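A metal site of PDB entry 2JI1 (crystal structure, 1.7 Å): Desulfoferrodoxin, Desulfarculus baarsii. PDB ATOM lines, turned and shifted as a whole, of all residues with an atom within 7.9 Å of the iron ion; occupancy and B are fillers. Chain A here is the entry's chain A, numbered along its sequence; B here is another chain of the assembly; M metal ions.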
ATOM      1  N   LYS A   9     -16.621  22.835 -15.752  1.00  0.00           N
ATOM      2  CA  LYS A   9     -16.364  23.391 -17.077  1.00  0.00           C
ATOM      3  C   LYS A   9     -16.104  24.885 -17.051  1.00  0.00           C
ATOM      4  O   LYS A   9     -16.732  25.629 -16.289  1.00  0.00           O
ATOM      5  CB  LYS A   9     -17.574  23.141 -17.990  1.00  0.00           C
ATOM      6  CG  LYS A   9     -17.491  23.876 -19.331  1.00  0.00           C
ATOM      7  CD  LYS A   9     -18.755  23.726 -20.159  1.00  0.00           C
ATOM      8  CE  LYS A   9     -18.621  24.446 -21.498  1.00  0.00           C
ATOM      9  NZ  LYS A   9     -19.819  24.265 -22.374  1.00  0.00           N
ATOM     10  N   CYS A  10     -15.156  25.328 -17.879  1.00  0.00           N
ATOM     11  CA  CYS A  10     -14.879  26.751 -17.986  1.00  0.00           C
ATOM     12  C   CYS A  10     -15.787  27.208 -19.123  1.00  0.00           C
ATOM     13  O   CYS A  10     -15.616  26.785 -20.262  1.00  0.00           O
ATOM     14  CB  CYS A  10     -13.426  27.030 -18.366  1.00  0.00           C
ATOM     15  SG  CYS A  10     -13.160  28.795 -18.642  1.00  0.00           S
ATOM     16  N   GLU A  11     -16.757  28.057 -18.818  1.00  0.00           N
ATOM     17  CA  GLU A  11     -17.677  28.523 -19.838  1.00  0.00           C
ATOM     18  C   GLU A  11     -17.043  29.473 -20.849  1.00  0.00           C
ATOM     19  O   GLU A  11     -17.648  29.799 -21.868  1.00  0.00           O
ATOM     20  CB  GLU A  11     -18.908  29.181 -19.183  1.00  0.00           C
ATOM     21  CG  GLU A  11     -19.754  28.184 -18.399  1.00  0.00           C
ATOM     22  CD  GLU A  11     -21.058  28.773 -17.895  1.00  0.00           C
ATOM     23  OE1 GLU A  11     -21.029  29.615 -16.972  1.00  0.00           O
ATOM     24  OE2 GLU A  11     -22.116  28.387 -18.432  1.00  0.00           O
ATOM     25  N   VAL A  12     -15.824  29.908 -20.573  1.00  0.00           N
ATOM     26  CA  VAL A  12     -15.128  30.811 -21.489  1.00  0.00           C
ATOM     27  C   VAL A  12     -14.319  30.049 -22.545  1.00  0.00           C
ATOM     28  O   VAL A  12     -14.592  30.177 -23.738  1.00  0.00           O
ATOM     29  CB  VAL A  12     -14.192  31.772 -20.733  1.00  0.00           C
ATOM     30  CG1 VAL A  12     -13.449  32.654 -21.719  1.00  0.00           C
ATOM     31  CG2 VAL A  12     -14.993  32.620 -19.762  1.00  0.00           C
ATOM     32  N   CYS A  13     -13.339  29.263 -22.106  1.00  0.00           N
ATOM     33  CA  CYS A  13     -12.490  28.518 -23.047  1.00  0.00           C
ATOM     34  C   CYS A  13     -12.912  27.082 -23.345  1.00  0.00           C
ATOM     35  O   CYS A  13     -12.376  26.459 -24.254  1.00  0.00           O
ATOM     36  CB  CYS A  13     -11.041  28.523 -22.562  1.00  0.00           C
ATOM     37  SG  CYS A  13     -10.741  27.520 -21.112  1.00  0.00           S
ATOM     38  N   GLY A  14     -13.842  26.551 -22.575  1.00  0.00           N
ATOM     39  CA  GLY A  14     -14.287  25.198 -22.841  1.00  0.00           C
ATOM     40  C   GLY A  14     -13.592  24.069 -22.085  1.00  0.00           C
ATOM     41  O   GLY A  14     -13.940  22.913 -22.282  1.00  0.00           O
ATOM     42  N   ASN A  15     -12.609  24.389 -21.246  1.00  0.00           N
ATOM     43  CA  ASN A  15     -11.933  23.347 -20.474  1.00  0.00           C
ATOM     44  C   ASN A  15     -12.976  22.623 -19.641  1.00  0.00           C
ATOM     45  O   ASN A  15     -13.876  23.248 -19.068  1.00  0.00           O
ATOM     46  CB  ASN A  15     -10.911  23.926 -19.481  1.00  0.00           C
ATOM     47  CG  ASN A  15      -9.577  24.271 -20.125  1.00  0.00           C
ATOM     48  OD1 ASN A  15      -9.246  23.787 -21.211  1.00  0.00           O
ATOM     49  ND2 ASN A  15      -8.781  25.075 -19.425  1.00  0.00           N
ATOM     50  N   ILE A  16     -12.880  21.306 -19.576  1.00  0.00           N
ATOM     51  CA  ILE A  16     -13.778  20.513 -18.752  1.00  0.00           C
ATOM     52  C   ILE A  16     -12.857  19.524 -18.059  1.00  0.00           C
ATOM     53  O   ILE A  16     -12.027  18.869 -18.694  1.00  0.00           O
ATOM     54  CB  ILE A  16     -14.813  19.721 -19.569  1.00  0.00           C
ATOM     55  CG1 ILE A  16     -15.721  20.692 -20.327  1.00  0.00           C
ATOM     56  CG2 ILE A  16     -15.654  18.852 -18.629  1.00  0.00           C
ATOM     57  CD1 ILE A  16     -16.728  19.997 -21.226  1.00  0.00           C
ATOM     58  N   VAL A  28     -10.729  27.567 -10.808  1.00  0.00           N
ATOM     59  CA  VAL A  28     -10.904  28.782 -11.583  1.00  0.00           C
ATOM     60  C   VAL A  28     -10.256  28.679 -12.956  1.00  0.00           C
ATOM     61  O   VAL A  28      -9.213  28.043 -13.118  1.00  0.00           O
ATOM     62  CB  VAL A  28     -10.293  29.995 -10.841  1.00  0.00           C
ATOM     63  CG1 VAL A  28     -10.380  31.249 -11.682  1.00  0.00           C
ATOM     64  CG2 VAL A  28     -11.016  30.184  -9.517  1.00  0.00           C
ATOM     65  N   CYS A  29     -10.874  29.301 -13.960  1.00  0.00           N
ATOM     66  CA  CYS A  29     -10.336  29.309 -15.308  1.00  0.00           C
ATOM     67  C   CYS A  29     -10.857  30.550 -16.020  1.00  0.00           C
ATOM     68  O   CYS A  29     -12.015  30.936 -15.848  1.00  0.00           O
ATOM     69  CB  CYS A  29     -10.749  28.058 -16.082  1.00  0.00           C
ATOM     70  SG  CYS A  29      -9.794  27.783 -17.607  1.00  0.00           S
ATOM     71  N   CYS A  30      -9.990  31.183 -16.800  1.00  0.00           N
ATOM     72  CA  CYS A  30     -10.354  32.381 -17.535  1.00  0.00           C
ATOM     73  C   CYS A  30     -11.001  33.448 -16.653  1.00  0.00           C
ATOM     74  O   CYS A  30     -12.032  34.028 -16.992  1.00  0.00           O
ATOM     75  CB  CYS A  30     -11.276  32.010 -18.702  1.00  0.00           C
ATOM     76  SG  CYS A  30     -10.448  30.994 -19.951  1.00  0.00           S
ATOM     77  N   ASN A  31     -10.380  33.676 -15.498  1.00  0.00           N
ATOM     78  CA  ASN A  31     -10.803  34.692 -14.531  1.00  0.00           C
ATOM     79  C   ASN A  31     -12.156  34.502 -13.871  1.00  0.00           C
ATOM     80  O   ASN A  31     -12.713  35.464 -13.325  1.00  0.00           O
ATOM     81  CB  ASN A  31     -10.756  36.066 -15.198  1.00  0.00           C
ATOM     82  CG  ASN A  31      -9.432  36.309 -15.893  1.00  0.00           C
ATOM     83  OD1 ASN A  31      -9.384  36.470 -17.114  1.00  0.00           O
ATOM     84  ND2 ASN A  31      -8.356  36.330 -15.118  1.00  0.00           N
ATOM     85  N   GLN A  32     -12.702  33.296 -13.903  1.00  0.00           N
ATOM     86  CA  GLN A  32     -13.992  33.060 -13.266  1.00  0.00           C
ATOM     87  C   GLN A  32     -14.086  31.627 -12.770  1.00  0.00           C
ATOM     88  O   GLN A  32     -13.385  30.740 -13.259  1.00  0.00           O
ATOM     89  CB  GLN A  32     -15.140  33.372 -14.227  1.00  0.00           C
ATOM     90  CG  GLN A  32     -15.239  32.454 -15.437  1.00  0.00           C
ATOM     91  CD  GLN A  32     -16.348  32.881 -16.397  1.00  0.00           C
ATOM     92  OE1 GLN A  32     -17.131  32.051 -16.860  1.00  0.00           O
ATOM     93  NE2 GLN A  32     -16.411  34.169 -16.709  1.00  0.00           N
ATOM     94  N   MET A  34     -15.044  27.915 -12.261  1.00  0.00           N
ATOM     95  CA  MET A  34     -15.468  26.916 -13.228  1.00  0.00           C
ATOM     96  C   MET A  34     -16.839  26.459 -12.775  1.00  0.00           C
ATOM     97  O   MET A  34     -17.118  26.374 -11.577  1.00  0.00           O
ATOM     98  CB  MET A  34     -14.483  25.732 -13.251  1.00  0.00           C
ATOM     99  CG  MET A  34     -13.152  26.086 -13.874  1.00  0.00           C
ATOM    100  SD  MET A  34     -12.042  24.674 -14.031  1.00  0.00           S
ATOM    101  CE  MET A  34     -12.631  23.927 -15.584  1.00  0.00           C
ATOM    102  N   PRO B   2      -4.787  23.319 -21.880  1.00  0.00           N
ATOM    103  CA  PRO B   2      -4.601  21.903 -21.482  1.00  0.00           C
ATOM    104  C   PRO B   2      -5.209  20.925 -22.483  1.00  0.00           C
ATOM    105  O   PRO B   2      -6.026  21.307 -23.335  1.00  0.00           O
ATOM    106  CB  PRO B   2      -5.224  21.737 -20.096  1.00  0.00           C
ATOM    107  CG  PRO B   2      -6.139  22.950 -20.011  1.00  0.00           C
ATOM    108  CD  PRO B   2      -5.396  24.056 -20.763  1.00  0.00           C
ATOM    109  N   GLY B  23      -8.732  22.980 -23.795  1.00  0.00           N
ATOM    110  CA  GLY B  23      -9.046  24.363 -24.086  1.00  0.00           C
ATOM    111  C   GLY B  23      -7.766  25.160 -23.935  1.00  0.00           C
ATOM    112  O   GLY B  23      -6.722  24.605 -23.610  1.00  0.00           O
ATOM    113  N   ILE B  24      -7.826  26.474 -24.165  1.00  0.00           N
ATOM    114  CA  ILE B  24      -6.632  27.299 -24.065  1.00  0.00           C
ATOM    115  C   ILE B  24      -6.413  27.941 -22.702  1.00  0.00           C
ATOM    116  O   ILE B  24      -5.333  28.463 -22.429  1.00  0.00           O
ATOM    117  CB  ILE B  24      -6.647  28.418 -25.138  1.00  0.00           C
ATOM    118  CG1 ILE B  24      -7.847  29.342 -24.899  1.00  0.00           C
ATOM    119  CG2 ILE B  24      -6.713  27.815 -26.525  1.00  0.00           C
ATOM    120  CD1 ILE B  24      -7.920  30.524 -25.845  1.00  0.00           C
ATOM    121  N   GLY B  25      -7.425  27.910 -21.843  1.00  0.00           N
ATOM    122  CA  GLY B  25      -7.291  28.537 -20.537  1.00  0.00           C
ATOM    123  C   GLY B  25      -6.426  27.783 -19.554  1.00  0.00           C
ATOM    124  O   GLY B  25      -6.420  26.557 -19.523  1.00  0.00           O
ATOM    125  N   GLU B  26      -5.678  28.518 -18.738  1.00  0.00           N
ATOM    126  CA  GLU B  26      -4.828  27.888 -17.741  1.00  0.00           C
ATOM    127  C   GLU B  26      -5.648  27.627 -16.487  1.00  0.00           C
ATOM    128  O   GLU B  26      -6.248  28.537 -15.924  1.00  0.00           O
ATOM    129  CB  GLU B  26      -3.623  28.774 -17.392  1.00  0.00           C
ATOM    130  CG  GLU B  26      -2.535  28.795 -18.457  1.00  0.00           C
ATOM    131  N   LEU B  27      -5.683  26.365 -16.056  1.00  0.00           N
ATOM    132  CA  LEU B  27      -6.428  25.994 -14.865  1.00  0.00           C
ATOM    133  C   LEU B  27      -5.777  26.647 -13.646  1.00  0.00           C
ATOM    134  O   LEU B  27      -4.569  26.590 -13.467  1.00  0.00           O
ATOM    135  CB  LEU B  27      -6.435  24.476 -14.694  1.00  0.00           C
ATOM    136  CG  LEU B  27      -7.156  23.726 -15.817  1.00  0.00           C
ATOM    137  CD1 LEU B  27      -6.906  22.231 -15.662  1.00  0.00           C
ATOM    138  CD2 LEU B  27      -8.649  24.040 -15.768  1.00  0.00           C
HETATM  139 FE    FE M   1     -11.013  28.814 -19.290  1.00  0.00          FE
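The backbone NH (N) of Cys 10 sits at hydrogen-bond distance from the backbone carbonyl oxygen (O) of Asn 15 (2.7 Å). The side-chain sulfur (SG) of Cys 10 lies close to the backbone NH (N) of Val 12 (3.5 Å). SG of Cys 13 sits close to N of Gly 25 of chain B (3.4 Å). The side-chain amide nitrogen (ND2) of Asn 15 sits close to the side-chain sulfur (SG) of Cys 13. The side-chain sulfur (SG) of Cys 29 lies close to the side-chain amide nitrogen (ND2) of Asn 15, at 3.4 Å. ND2 of Asn 15 is in hydrogen-bond range of O of Gly 25 of chain B.
Gly 25 of chain B touches the iron ion (CA to FE, 3.9 Å). Along chain A the residues within 4 Å of the iron ion span positions 10 to 30.
The side-chain sulfur (SG) of Cys 10 binds the iron ion (2.2 Å). SG of Cys 13 binds the iron ion (2.3 Å). SG of Cys 29 binds the iron ion. SG of Cys 30 binds the iron ion, at 2.3 Å.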
